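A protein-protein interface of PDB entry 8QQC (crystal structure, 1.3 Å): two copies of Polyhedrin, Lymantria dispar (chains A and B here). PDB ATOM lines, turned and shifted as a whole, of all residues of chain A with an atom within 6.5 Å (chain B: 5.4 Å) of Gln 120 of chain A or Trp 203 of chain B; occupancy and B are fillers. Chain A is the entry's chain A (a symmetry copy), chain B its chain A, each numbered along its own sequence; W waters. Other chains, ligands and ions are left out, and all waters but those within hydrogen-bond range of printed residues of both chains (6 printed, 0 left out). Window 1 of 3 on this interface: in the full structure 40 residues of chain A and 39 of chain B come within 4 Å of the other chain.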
ATOM      1  N   GLU A  54     -30.124 -15.965 -19.668  1.00  0.00           N
ATOM      2  CA  GLU A  54     -30.239 -14.627 -19.112  1.00  0.00           C
ATOM      3  C   GLU A  54     -29.867 -13.595 -20.162  1.00  0.00           C
ATOM      4  O   GLU A  54     -29.023 -13.841 -21.029  1.00  0.00           O
ATOM      5  CB  GLU A  54     -29.311 -14.448 -17.899  1.00  0.00           C
ATOM      6  CG  GLU A  54     -29.543 -15.418 -16.731  1.00  0.00           C
ATOM      7  CD  GLU A  54     -30.843 -15.169 -15.990  1.00  0.00           C
ATOM      8  OE1 GLU A  54     -31.419 -14.070 -16.128  1.00  0.00           O
ATOM      9  OE2 GLU A  54     -31.291 -16.084 -15.262  1.00  0.00           O
ATOM     10  N   THR A  55     -30.513 -12.433 -20.072  1.00  0.00           N
ATOM     11  CA  THR A  55     -30.069 -11.219 -20.746  1.00  0.00           C
ATOM     12  C   THR A  55     -29.465 -10.285 -19.709  1.00  0.00           C
ATOM     13  O   THR A  55     -30.052 -10.071 -18.641  1.00  0.00           O
ATOM     14  CB  THR A  55     -31.229 -10.499 -21.440  1.00  0.00           C
ATOM     15  OG1 THR A  55     -31.814 -11.345 -22.436  1.00  0.00           O
ATOM     16  CG2 THR A  55     -30.733  -9.229 -22.113  1.00  0.00           C
ATOM     17  N   LEU A  56     -28.294  -9.739 -20.018  1.00  0.00           N
ATOM     18  CA  LEU A  56     -27.719  -8.622 -19.278  1.00  0.00           C
ATOM     19  C   LEU A  56     -27.895  -7.389 -20.158  1.00  0.00           C
ATOM     20  O   LEU A  56     -27.225  -7.258 -21.188  1.00  0.00           O
ATOM     21  CB  LEU A  56     -26.250  -8.881 -18.946  1.00  0.00           C
ATOM     22  CG  LEU A  56     -25.988 -10.078 -18.024  1.00  0.00           C
ATOM     23  CD1 LEU A  56     -24.496 -10.302 -17.807  1.00  0.00           C
ATOM     24  CD2 LEU A  56     -26.713  -9.929 -16.679  1.00  0.00           C
ATOM     25  N   ASN A 118     -23.693 -14.009 -26.553  1.00  0.00           N
ATOM     26  CA  ASN A 118     -24.108 -13.205 -27.696  1.00  0.00           C
ATOM     27  C   ASN A 118     -24.116 -11.749 -27.239  1.00  0.00           C
ATOM     28  O   ASN A 118     -25.041 -11.311 -26.547  1.00  0.00           O
ATOM     29  CB  ASN A 118     -25.483 -13.670 -28.168  1.00  0.00           C
ATOM     30  CG  ASN A 118     -25.976 -12.922 -29.393  1.00  0.00           C
ATOM     31  OD1 ASN A 118     -25.403 -11.909 -29.802  1.00  0.00           O
ATOM     32  ND2 ASN A 118     -27.050 -13.428 -29.991  1.00  0.00           N
ATOM     33  N   ILE A 119     -23.083 -11.009 -27.633  1.00  0.00           N
ATOM     34  CA  ILE A 119     -22.916  -9.609 -27.260  1.00  0.00           C
ATOM     35  C   ILE A 119     -23.375  -8.739 -28.422  1.00  0.00           C
ATOM     36  O   ILE A 119     -22.880  -8.873 -29.548  1.00  0.00           O
ATOM     37  CB  ILE A 119     -21.462  -9.292 -26.874  1.00  0.00           C
ATOM     38  CG1 ILE A 119     -20.989 -10.233 -25.766  1.00  0.00           C
ATOM     39  CG2 ILE A 119     -21.348  -7.846 -26.404  1.00  0.00           C
ATOM     40  CD1 ILE A 119     -19.549  -9.994 -25.345  1.00  0.00           C
ATOM     41  N   GLN A 120     -24.313  -7.846 -28.151  1.00  0.00           N
ATOM     42  CA  GLN A 120     -24.826  -6.922 -29.150  1.00  0.00           C
ATOM     43  C   GLN A 120     -24.615  -5.489 -28.677  1.00  0.00           C
ATOM     44  O   GLN A 120     -24.115  -5.235 -27.574  1.00  0.00           O
ATOM     45  CB  GLN A 120     -26.310  -7.190 -29.429  1.00  0.00           C
ATOM     46  CG  GLN A 120     -26.577  -8.544 -30.072  1.00  0.00           C
ATOM     47  CD  GLN A 120     -25.935  -8.681 -31.439  1.00  0.00           C
ATOM     48  OE1 GLN A 120     -25.842  -7.712 -32.195  1.00  0.00           O
ATOM     49  NE2 GLN A 120     -25.465  -9.886 -31.755  1.00  0.00           N
ATOM     50  N   GLY A 121     -24.975  -4.547 -29.542  1.00  0.00           N
ATOM     51  CA  GLY A 121     -25.060  -3.157 -29.168  1.00  0.00           C
ATOM     52  C   GLY A 121     -26.297  -2.877 -28.340  1.00  0.00           C
ATOM     53  O   GLY A 121     -27.020  -3.775 -27.903  1.00  0.00           O
ATOM     54  N   TYR A 122     -26.547  -1.580 -28.141  1.00  0.00           N
ATOM     55  CA  TYR A 122     -27.598  -1.137 -27.229  1.00  0.00           C
ATOM     56  C   TYR A 122     -28.971  -1.666 -27.620  1.00  0.00           C
ATOM     57  O   TYR A 122     -29.791  -1.960 -26.745  1.00  0.00           O
ATOM     58  CB  TYR A 122     -27.616   0.389 -27.176  1.00  0.00           C
ATOM     59  CG  TYR A 122     -28.598   0.968 -26.182  1.00  0.00           C
ATOM     60  CD1 TYR A 122     -28.306   0.986 -24.822  1.00  0.00           C
ATOM     61  CD2 TYR A 122     -29.808   1.506 -26.601  1.00  0.00           C
ATOM     62  CE1 TYR A 122     -29.196   1.525 -23.900  1.00  0.00           C
ATOM     63  CE2 TYR A 122     -30.703   2.046 -25.689  1.00  0.00           C
ATOM     64  CZ  TYR A 122     -30.391   2.051 -24.341  1.00  0.00           C
ATOM     65  OH  TYR A 122     -31.278   2.585 -23.433  1.00  0.00           O
ATOM     66  N   ASP A 123     -29.243  -1.802 -28.919  1.00  0.00           N
ATOM     67  CA  ASP A 123     -30.577  -2.191 -29.363  1.00  0.00           C
ATOM     68  C   ASP A 123     -30.822  -3.698 -29.359  1.00  0.00           C
ATOM     69  O   ASP A 123     -31.958  -4.111 -29.612  1.00  0.00           O
ATOM     70  CB  ASP A 123     -30.866  -1.644 -30.763  1.00  0.00           C
ATOM     71  CG  ASP A 123     -30.917  -0.128 -30.811  1.00  0.00           C
ATOM     72  OD1 ASP A 123     -31.062   0.508 -29.748  1.00  0.00           O
ATOM     73  OD2 ASP A 123     -30.830   0.420 -31.932  1.00  0.00           O
ATOM     74  N   GLU A 124     -29.804  -4.520 -29.095  1.00  0.00           N
ATOM     75  CA  GLU A 124     -29.913  -5.977 -29.025  1.00  0.00           C
ATOM     76  C   GLU A 124     -30.241  -6.635 -30.362  1.00  0.00           C
ATOM     77  O   GLU A 124     -30.580  -7.826 -30.388  1.00  0.00           O
ATOM     78  CB  GLU A 124     -30.917  -6.440 -27.955  1.00  0.00           C
ATOM     79  CG  GLU A 124     -30.656  -5.862 -26.573  1.00  0.00           C
ATOM     80  CD  GLU A 124     -31.650  -6.343 -25.529  1.00  0.00           C
ATOM     81  OE1 GLU A 124     -32.750  -6.812 -25.901  1.00  0.00           O
ATOM     82  OE2 GLU A 124     -31.328  -6.242 -24.325  1.00  0.00           O
ATOM     83  N   ILE A 125     -30.160  -5.909 -31.473  1.00  0.00           N
ATOM     84  CA  ILE A 125     -30.631  -6.408 -32.761  1.00  0.00           C
ATOM     85  C   ILE A 125     -29.427  -6.794 -33.610  1.00  0.00           C
ATOM     86  O   ILE A 125     -28.649  -5.932 -34.034  1.00  0.00           O
ATOM     87  CB  ILE A 125     -31.527  -5.385 -33.467  1.00  0.00           C
ATOM     88  CG1 ILE A 125     -32.829  -5.210 -32.685  1.00  0.00           C
ATOM     89  CG2 ILE A 125     -31.801  -5.826 -34.902  1.00  0.00           C
ATOM     90  CD1 ILE A 125     -33.581  -3.936 -33.008  1.00  0.00           C
ATOM     91  N   GLU A 126     -29.284  -8.089 -33.881  1.00  0.00           N
ATOM     92  CA  GLU A 126     -28.171  -8.579 -34.680  1.00  0.00           C
ATOM     93  C   GLU A 126     -28.418  -8.259 -36.149  1.00  0.00           C
ATOM     94  O   GLU A 126     -29.544  -8.365 -36.647  1.00  0.00           O
ATOM     95  CB  GLU A 126     -28.058 -10.095 -34.519  1.00  0.00           C
ATOM     96  CG  GLU A 126     -26.820 -10.742 -35.153  1.00  0.00           C
ATOM     97  CD  GLU A 126     -26.927 -10.944 -36.653  1.00  0.00           C
ATOM     98  OE1 GLU A 126     -28.027 -11.268 -37.143  1.00  0.00           O
ATOM     99  OE2 GLU A 126     -25.890 -10.810 -37.345  1.00  0.00           O
ATOM    100  N   GLY A 127     -27.358  -7.880 -36.846  1.00  0.00           N
ATOM    101  CA  GLY A 127     -27.452  -7.689 -38.280  1.00  0.00           C
ATOM    102  C   GLY A 127     -28.097  -6.372 -38.682  1.00  0.00           C
ATOM    103  O   GLY A 127     -28.205  -5.419 -37.902  1.00  0.00           O
ATOM    104  N   ASN A 134     -30.045 -13.129 -36.998  1.00  0.00           N
ATOM    105  CA  ASN A 134     -29.819 -14.542 -36.756  1.00  0.00           C
ATOM    106  C   ASN A 134     -29.828 -14.797 -35.258  1.00  0.00           C
ATOM    107  O   ASN A 134     -29.253 -14.024 -34.486  1.00  0.00           O
ATOM    108  CB  ASN A 134     -28.472 -14.972 -37.327  1.00  0.00           C
ATOM    109  CG  ASN A 134     -28.452 -14.943 -38.830  1.00  0.00           C
ATOM    110  OD1 ASN A 134     -29.451 -15.245 -39.481  1.00  0.00           O
ATOM    111  ND2 ASN A 134     -27.306 -14.581 -39.396  1.00  0.00           N
ATOM    112  N   VAL A 135     -30.488 -15.885 -34.857  1.00  0.00           N
ATOM    113  CA  VAL A 135     -30.520 -16.264 -33.445  1.00  0.00           C
ATOM    114  C   VAL A 135     -29.135 -16.646 -32.942  1.00  0.00           C
ATOM    115  O   VAL A 135     -28.824 -16.456 -31.760  1.00  0.00           O
ATOM    116  CB  VAL A 135     -31.558 -17.374 -33.193  1.00  0.00           C
ATOM    117  CG1 VAL A 135     -32.958 -16.860 -33.511  1.00  0.00           C
ATOM    118  CG2 VAL A 135     -31.235 -18.619 -34.016  1.00  0.00           C
ATOM    119  N   PRO A 137     -25.510 -15.733 -34.201  1.00  0.00           N
ATOM    120  CA  PRO A 137     -24.419 -15.194 -35.006  1.00  0.00           C
ATOM    121  C   PRO A 137     -23.144 -15.964 -34.723  1.00  0.00           C
ATOM    122  O   PRO A 137     -22.968 -16.515 -33.621  1.00  0.00           O
ATOM    123  CB  PRO A 137     -24.313 -13.733 -34.528  1.00  0.00           C
ATOM    124  CG  PRO A 137     -24.943 -13.720 -33.172  1.00  0.00           C
ATOM    125  CD  PRO A 137     -25.996 -14.784 -33.182  1.00  0.00           C
ATOM    126  N   TYR A 139     -20.128 -15.309 -33.882  1.00  0.00           N
ATOM    127  CA  TYR A 139     -19.367 -14.934 -32.697  1.00  0.00           C
ATOM    128  C   TYR A 139     -20.051 -15.331 -31.397  1.00  0.00           C
ATOM    129  O   TYR A 139     -19.424 -15.230 -30.338  1.00  0.00           O
ATOM    130  CB  TYR A 139     -19.063 -13.437 -32.712  1.00  0.00           C
ATOM    131  CG  TYR A 139     -20.247 -12.567 -33.061  1.00  0.00           C
ATOM    132  CD1 TYR A 139     -21.230 -12.293 -32.123  1.00  0.00           C
ATOM    133  CD2 TYR A 139     -20.384 -12.026 -34.333  1.00  0.00           C
ATOM    134  CE1 TYR A 139     -22.313 -11.494 -32.436  1.00  0.00           C
ATOM    135  CE2 TYR A 139     -21.466 -11.225 -34.659  1.00  0.00           C
ATOM    136  CZ  TYR A 139     -22.428 -10.965 -33.707  1.00  0.00           C
ATOM    137  OH  TYR A 139     -23.509 -10.168 -34.019  1.00  0.00           O
ATOM    138  N   ASP A 167     -20.026  -0.231 -31.497  1.00  0.00           N
ATOM    139  CA  ASP A 167     -21.373  -0.566 -31.036  1.00  0.00           C
ATOM    140  C   ASP A 167     -21.360  -1.411 -29.767  1.00  0.00           C
ATOM    141  O   ASP A 167     -22.173  -1.186 -28.862  1.00  0.00           O
ATOM    142  CB  ASP A 167     -22.172  -1.272 -32.135  1.00  0.00           C
ATOM    143  CG  ASP A 167     -22.551  -0.349 -33.278  1.00  0.00           C
ATOM    144  OD1 ASP A 167     -22.442   0.882 -33.110  1.00  0.00           O
ATOM    145  OD2 ASP A 167     -22.956  -0.857 -34.347  1.00  0.00           O
ATOM    146  N   ARG A 168     -20.461  -2.390 -29.681  1.00  0.00           N
ATOM    147  CA  ARG A 168     -20.439  -3.247 -28.503  1.00  0.00           C
ATOM    148  C   ARG A 168     -19.799  -2.572 -27.297  1.00  0.00           C
ATOM    149  O   ARG A 168     -19.786  -3.157 -26.211  1.00  0.00           O
ATOM    150  CB  ARG A 168     -19.766  -4.586 -28.810  1.00  0.00           C
ATOM    151  CG  ARG A 168     -20.602  -5.453 -29.726  1.00  0.00           C
ATOM    152  CD  ARG A 168     -19.935  -6.794 -29.995  1.00  0.00           C
ATOM    153  NE  ARG A 168     -20.823  -7.674 -30.741  1.00  0.00           N
ATOM    154  CZ  ARG A 168     -21.268  -7.436 -31.968  1.00  0.00           C
ATOM    155  NH1 ARG A 168     -20.766  -6.463 -32.711  1.00  0.00           N
ATOM    156  NH2 ARG A 168     -22.227  -8.208 -32.469  1.00  0.00           N
ATOM    157  N   GLY A 169     -19.268  -1.363 -27.466  1.00  0.00           N
ATOM    158  CA  GLY A 169     -18.942  -0.521 -26.332  1.00  0.00           C
ATOM    159  C   GLY A 169     -20.151   0.000 -25.588  1.00  0.00           C
ATOM    160  O   GLY A 169     -19.987   0.615 -24.530  1.00  0.00           O
ATOM    161  N   HIS A 170     -21.354  -0.217 -26.122  1.00  0.00           N
ATOM    162  CA  HIS A 170     -22.611   0.061 -25.432  1.00  0.00           C
ATOM    163  C   HIS A 170     -23.347  -1.270 -25.364  1.00  0.00           C
ATOM    164  O   HIS A 170     -24.361  -1.472 -26.048  1.00  0.00           O
ATOM    165  CB  HIS A 170     -23.435   1.096 -26.197  1.00  0.00           C
ATOM    166  CG  HIS A 170     -22.606   2.171 -26.827  1.00  0.00           C
ATOM    167  ND1 HIS A 170     -21.991   3.162 -26.094  1.00  0.00           N
ATOM    168  CD2 HIS A 170     -22.274   2.400 -28.120  1.00  0.00           C
ATOM    169  CE1 HIS A 170     -21.316   3.956 -26.908  1.00  0.00           C
ATOM    170  NE2 HIS A 170     -21.476   3.518 -28.143  1.00  0.00           N
ATOM    171  N   PRO A 171     -22.855  -2.203 -24.553  1.00  0.00           N
ATOM    172  CA  PRO A 171     -23.178  -3.615 -24.768  1.00  0.00           C
ATOM    173  C   PRO A 171     -24.504  -4.056 -24.164  1.00  0.00           C
ATOM    174  O   PRO A 171     -25.036  -3.468 -23.219  1.00  0.00           O
ATOM    175  CB  PRO A 171     -22.021  -4.340 -24.077  1.00  0.00           C
ATOM    176  CG  PRO A 171     -21.624  -3.412 -22.974  1.00  0.00           C
ATOM    177  CD  PRO A 171     -21.825  -2.023 -23.510  1.00  0.00           C
ATOM    178  N   THR A 172     -25.035  -5.116 -24.770  1.00  0.00           N
ATOM    179  CA  THR A 172     -26.034  -5.996 -24.184  1.00  0.00           C
ATOM    180  C   THR A 172     -25.582  -7.424 -24.457  1.00  0.00           C
ATOM    181  O   THR A 172     -24.835  -7.683 -25.406  1.00  0.00           O
ATOM    182  CB  THR A 172     -27.430  -5.775 -24.789  1.00  0.00           C
ATOM    183  OG1 THR A 172     -27.388  -6.016 -26.201  1.00  0.00           O
ATOM    184  CG2 THR A 172     -27.922  -4.352 -24.518  1.00  0.00           C
ATOM    185  N   MET A 173     -26.028  -8.356 -23.615  1.00  0.00           N
ATOM    186  CA  MET A 173     -25.509  -9.719 -23.643  1.00  0.00           C
ATOM    187  C   MET A 173     -26.633 -10.707 -23.408  1.00  0.00           C
ATOM    188  O   MET A 173     -27.375 -10.565 -22.436  1.00  0.00           O
ATOM    189  CB  MET A 173     -24.567  -9.952 -22.470  1.00  0.00           C
ATOM    190  CG  MET A 173     -23.673 -11.137 -22.646  1.00  0.00           C
ATOM    191  SD  MET A 173     -22.357 -11.076 -21.439  1.00  0.00           S
ATOM    192  CE  MET A 173     -21.452  -9.629 -21.968  1.00  0.00           C
ATOM    193  N   ALA A 174     -26.710 -11.743 -24.238  1.00  0.00           N
ATOM    194  CA  ALA A 174     -27.502 -12.930 -23.936  1.00  0.00           C
ATOM    195  C   ALA A 174     -26.549 -14.083 -23.657  1.00  0.00           C
ATOM    196  O   ALA A 174     -25.624 -14.326 -24.439  1.00  0.00           O
ATOM    197  CB  ALA A 174     -28.431 -13.275 -25.102  1.00  0.00           C
ATOM    198  N   TYR B  27     -35.753 -14.851 -35.298  1.00  0.00           N
ATOM    199  CA  TYR B  27     -36.544 -14.549 -34.115  1.00  0.00           C
ATOM    200  C   TYR B  27     -37.985 -14.244 -34.511  1.00  0.00           C
ATOM    201  O   TYR B  27     -38.270 -13.816 -35.632  1.00  0.00           O
ATOM    202  CB  TYR B  27     -35.992 -13.314 -33.397  1.00  0.00           C
ATOM    203  CG  TYR B  27     -34.657 -13.469 -32.709  1.00  0.00           C
ATOM    204  CD1 TYR B  27     -34.582 -13.931 -31.401  1.00  0.00           C
ATOM    205  CD2 TYR B  27     -33.474 -13.103 -33.346  1.00  0.00           C
ATOM    206  CE1 TYR B  27     -33.372 -14.053 -30.760  1.00  0.00           C
ATOM    207  CE2 TYR B  27     -32.255 -13.223 -32.708  1.00  0.00           C
ATOM    208  CZ  TYR B  27     -32.211 -13.698 -31.417  1.00  0.00           C
ATOM    209  OH  TYR B  27     -31.001 -13.822 -30.768  1.00  0.00           O
ATOM    210  N   LYS B  45     -39.561  -4.073 -27.152  1.00  0.00           N
ATOM    211  CA  LYS B  45     -39.268  -5.233 -27.983  1.00  0.00           C
ATOM    212  C   LYS B  45     -39.394  -6.484 -27.124  1.00  0.00           C
ATOM    213  O   LYS B  45     -38.708  -6.609 -26.102  1.00  0.00           O
ATOM    214  CB  LYS B  45     -37.842  -5.149 -28.529  1.00  0.00           C
ATOM    215  CG  LYS B  45     -37.335  -6.448 -29.167  1.00  0.00           C
ATOM    216  CD  LYS B  45     -35.994  -6.254 -29.855  1.00  0.00           C
ATOM    217  CE  LYS B  45     -34.886  -5.967 -28.849  1.00  0.00           C
ATOM    218  NZ  LYS B  45     -34.512  -7.189 -28.071  1.00  0.00           N
ATOM    219  N   THR B  47     -39.075 -10.635 -27.728  1.00  0.00           N
ATOM    220  CA  THR B  47     -38.472 -11.442 -28.781  1.00  0.00           C
ATOM    221  C   THR B  47     -37.954 -12.754 -28.214  1.00  0.00           C
ATOM    222  O   THR B  47     -37.576 -12.841 -27.042  1.00  0.00           O
ATOM    223  CB  THR B  47     -37.344 -10.693 -29.511  1.00  0.00           C
ATOM    224  OG1 THR B  47     -36.992 -11.406 -30.705  1.00  0.00           O
ATOM    225  CG2 THR B  47     -36.111 -10.578 -28.624  1.00  0.00           C
ATOM    226  N   ASN B  48     -37.929 -13.766 -29.070  1.00  0.00           N
ATOM    227  CA  ASN B  48     -37.487 -15.103 -28.698  1.00  0.00           C
ATOM    228  C   ASN B  48     -37.359 -15.923 -29.973  1.00  0.00           C
ATOM    229  O   ASN B  48     -38.019 -15.621 -30.970  1.00  0.00           O
ATOM    230  CB  ASN B  48     -38.497 -15.774 -27.756  1.00  0.00           C
ATOM    231  CG  ASN B  48     -37.934 -17.007 -27.091  1.00  0.00           C
ATOM    232  OD1 ASN B  48     -38.131 -18.132 -27.564  1.00  0.00           O
ATOM    233  ND2 ASN B  48     -37.208 -16.805 -25.998  1.00  0.00           N
ATOM    234  N   GLU B  54     -44.178 -12.422 -21.801  1.00  0.00           N
ATOM    235  CA  GLU B  54     -43.700 -11.273 -21.052  1.00  0.00           C
ATOM    236  C   GLU B  54     -44.856 -10.610 -20.323  1.00  0.00           C
ATOM    237  O   GLU B  54     -45.997 -10.618 -20.795  1.00  0.00           O
ATOM    238  CB  GLU B  54     -43.048 -10.236 -21.980  1.00  0.00           C
ATOM    239  CG  GLU B  54     -41.853 -10.736 -22.806  1.00  0.00           C
ATOM    240  CD  GLU B  54     -40.619 -11.017 -21.971  1.00  0.00           C
ATOM    241  OE1 GLU B  54     -40.537 -10.528 -20.825  1.00  0.00           O
ATOM    242  OE2 GLU B  54     -39.720 -11.735 -22.468  1.00  0.00           O
ATOM    243  N   ARG B 199     -32.819 -20.943 -24.285  1.00  0.00           N
ATOM    244  CA  ARG B 199     -32.983 -19.632 -24.893  1.00  0.00           C
ATOM    245  C   ARG B 199     -34.279 -18.952 -24.458  1.00  0.00           C
ATOM    246  O   ARG B 199     -34.768 -18.042 -25.141  1.00  0.00           O
ATOM    247  CB  ARG B 199     -32.866 -19.744 -26.413  1.00  0.00           C
ATOM    248  CG  ARG B 199     -31.616 -20.507 -26.835  1.00  0.00           C
ATOM    249  CD  ARG B 199     -31.395 -20.507 -28.334  1.00  0.00           C
ATOM    250  NE  ARG B 199     -32.351 -21.351 -29.042  1.00  0.00           N
ATOM    251  CZ  ARG B 199     -32.407 -21.464 -30.363  1.00  0.00           C
ATOM    252  NH1 ARG B 199     -31.578 -20.800 -31.149  1.00  0.00           N
ATOM    253  NH2 ARG B 199     -33.315 -22.266 -30.908  1.00  0.00           N
ATOM    254  N   ASN B 201     -34.781 -16.803 -22.290  1.00  0.00           N
ATOM    255  CA  ASN B 201     -34.558 -15.391 -22.015  1.00  0.00           C
ATOM    256  C   ASN B 201     -33.667 -14.731 -23.066  1.00  0.00           C
ATOM    257  O   ASN B 201     -32.954 -13.770 -22.764  1.00  0.00           O
ATOM    258  CB  ASN B 201     -33.987 -15.189 -20.613  1.00  0.00           C
ATOM    259  CG  ASN B 201     -35.018 -15.413 -19.536  1.00  0.00           C
ATOM    260  OD1 ASN B 201     -36.156 -14.964 -19.654  1.00  0.00           O
ATOM    261  ND2 ASN B 201     -34.632 -16.119 -18.482  1.00  0.00           N
ATOM    262  N   PHE B 202     -33.682 -15.250 -24.296  1.00  0.00           N
ATOM    263  CA  PHE B 202     -33.040 -14.604 -25.442  1.00  0.00           C
ATOM    264  C   PHE B 202     -34.181 -14.001 -26.258  1.00  0.00           C
ATOM    265  O   PHE B 202     -34.715 -14.644 -27.158  1.00  0.00           O
ATOM    266  CB  PHE B 202     -32.302 -15.619 -26.315  1.00  0.00           C
ATOM    267  CG  PHE B 202     -31.088 -16.265 -25.680  1.00  0.00           C
ATOM    268  CD1 PHE B 202     -30.847 -16.212 -24.319  1.00  0.00           C
ATOM    269  CD2 PHE B 202     -30.186 -16.950 -26.485  1.00  0.00           C
ATOM    270  CE1 PHE B 202     -29.724 -16.829 -23.772  1.00  0.00           C
ATOM    271  CE2 PHE B 202     -29.066 -17.568 -25.947  1.00  0.00           C
ATOM    272  CZ  PHE B 202     -28.836 -17.505 -24.587  1.00  0.00           C
ATOM    273  N   TRP B 203     -34.543 -12.752 -25.975  1.00  0.00           N
ATOM    274  CA  TRP B 203     -33.932 -11.770 -25.091  1.00  0.00           C
ATOM    275  C   TRP B 203     -34.981 -11.263 -24.115  1.00  0.00           C
ATOM    276  O   TRP B 203     -36.173 -11.285 -24.409  1.00  0.00           O
ATOM    277  CB  TRP B 203     -33.437 -10.578 -25.917  1.00  0.00           C
ATOM    278  CG  TRP B 203     -32.303 -10.894 -26.838  1.00  0.00           C
ATOM    279  CD1 TRP B 203     -32.354 -11.657 -27.970  1.00  0.00           C
ATOM    280  CD2 TRP B 203     -30.947 -10.451 -26.715  1.00  0.00           C
ATOM    281  NE1 TRP B 203     -31.112 -11.725 -28.553  1.00  0.00           N
ATOM    282  CE2 TRP B 203     -30.230 -10.992 -27.803  1.00  0.00           C
ATOM    283  CE3 TRP B 203     -30.266  -9.658 -25.786  1.00  0.00           C
ATOM    284  CZ2 TRP B 203     -28.869 -10.762 -27.987  1.00  0.00           C
ATOM    285  CZ3 TRP B 203     -28.919  -9.428 -25.975  1.00  0.00           C
ATOM    286  CH2 TRP B 203     -28.234  -9.980 -27.064  1.00  0.00           C
ATOM    287  N   ALA B 204     -34.535 -10.787 -22.959  1.00  0.00           N
ATOM    288  CA  ALA B 204     -35.453 -10.137 -22.037  1.00  0.00           C
ATOM    289  C   ALA B 204     -36.045  -8.888 -22.684  1.00  0.00           C
ATOM    290  O   ALA B 204     -35.465  -8.297 -23.600  1.00  0.00           O
ATOM    291  CB  ALA B 204     -34.722  -9.751 -20.754  1.00  0.00           C
ATOM    292  N   LYS B 205     -37.219  -8.485 -22.196  1.00  0.00           N
ATOM    293  CA  LYS B 205     -37.893  -7.321 -22.757  1.00  0.00           C
ATOM    294  C   LYS B 205     -36.979  -6.101 -22.713  1.00  0.00           C
ATOM    295  O   LYS B 205     -36.227  -5.897 -21.756  1.00  0.00           O
ATOM    296  CB  LYS B 205     -39.206  -7.043 -22.015  1.00  0.00           C
ATOM    297  CG  LYS B 205     -39.069  -6.817 -20.514  1.00  0.00           C
ATOM    298  CD  LYS B 205     -40.443  -6.674 -19.849  1.00  0.00           C
ATOM    299  CE  LYS B 205     -40.369  -6.907 -18.346  1.00  0.00           C
ATOM    300  NZ  LYS B 205     -39.800  -5.740 -17.622  1.00  0.00           N
HETATM  301  O   HOH W   1     -31.062 -16.496 -29.837  1.00  0.00           O
HETATM  302  O   HOH W   2     -29.677 -14.030 -28.596  1.00  0.00           O
HETATM  303  O   HOH W   3     -29.315 -18.996 -30.178  1.00  0.00           O
HETATM  304  O   HOH W   4     -33.209  -8.792 -30.030  1.00  0.00           O
HETATM  305  O   HOH W   5     -28.919 -12.566 -32.127  1.00  0.00           O
HETATM  306  O   HOH W   6     -33.941 -17.937 -16.146  1.00  0.00           O
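OE1 of Glu 124 of chain A lies within salt-bridge range of NZ of Lys 45 of chain B.
OG1 of Thr 55 of chain A lies within hydrogen-bond range of O of Asn 201 of chain B.
The backbone NH (N) of Ala 204 of chain B is in hydrogen-bond range of the side-chain hydroxyl (OG1) of Thr 55 of chain A, 2.8 Å away.
N of Leu 56 of chain A sits at hydrogen-bond distance from O of Met 173 of chain A, 2.7 Å away.
The side-chain amide oxygen (OD1) of Asn 118 of chain A is in hydrogen-bond range of the side-chain amide nitrogen (NE2) of Gln 120 of chain A, 2.8 Å away.
The backbone carbonyl oxygen (O) of Gly 121 of chain A is in hydrogen-bond range of the side-chain hydroxyl (OG1) of Thr 172 of chain A (2.8 Å).
Among the printed residues, merely in contact across the chains: Thr 55 of chain A with Trp 203 of chain B (3.4 Å), Asn 118 of chain A with Trp 203 of chain B (3.5 Å), Asp 123 of chain A with Lys 45 of chain B (3.5 Å), Val 135 of chain A with Tyr 27 of chain B (3.6 Å), Asn 134 of chain A with Tyr 27 of chain B (3.6 Å), Glu 124 of chain A with Trp 203 of chain B (3.6 Å), Val 135 of chain A with Arg 199 of chain B (3.6 Å), Ala 174 of chain A with Trp 203 of chain B (3.6 Å), Met 173 of chain A with Trp 203 of chain B (3.7 Å), Gln 120 of chain A with Trp 203 of chain B (3.7 Å), Thr 172 of chain A with Trp 203 of chain B (3.7 Å), Glu 124 of chain A with Ala 204 of chain B (3.9 Å) and Ala 174 of chain A with Phe 202 of chain B (3.9 Å).
Gln 120 of chain A touches one residue of chain B.
Of chain A, only Thr 55, Asn 118, Gln 120, Glu 124, Thr 172, Met 173 and Ala 174 come within 4 Å of Trp 203 of chain B.
Of the printed residues of chain B, Thr 172 of chain A touches Trp 203 (3.7 Å).
Of the printed residues of chain A, Tyr 27 of chain B touches Asn 134 and Val 135.
Of the printed residues of chain B, Asn 118 of chain A touches Trp 203 (3.5 Å).
Of the printed residues of chain B, Asp 123 of chain A touches Lys 45.
Arg 168 of chain A touches none of the printed residues of chain B.
Of the 25 printed residues of chain A, 10 touch a printed residue of chain B.
Printed residues of chain A that touch a printed residue of chain B: Thr 55, Asn 118, Gln 120, Asp 123, Glu 124, Asn 134, Val 135, Thr 172, Met 173 and Ala 174.
Of the 11 printed residues of chain B, 7 touch a printed residue of chain A.
Hydrophobic or aromatic side chains of chain B that line the printed part of chain A: Tyr 27, Phe 202, Trp 203 and Ala 204.
Among the printed residues, 16 pairs touch across the chains.
Among the printed residues, Asp or Glu carboxylates within 4 Å of a Lys or Arg side-chain nitrogen of the other chain: Glu 124 of chain A with Lys 45 of chain B.
1 position is printed for both chains.
Of the 16 pairs that touch across the chains among the printed residues, none has its exchanged pair printed and touching as well.
Water W2 lies within hydrogen-bond range of the side-chain hydroxyl (OH) of Tyr 27 of chain B (2.6 Å), the indole nitrogen (NE1) of Trp 203 of chain B (2.7 Å) and the side-chain amide nitrogen (ND2) of Asn 118 of chain A (3.0 Å).
Water W3 bridges the backbone carbonyl oxygen of Val 135 of chain A and the guanidinium group of Arg 199 of chain B.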
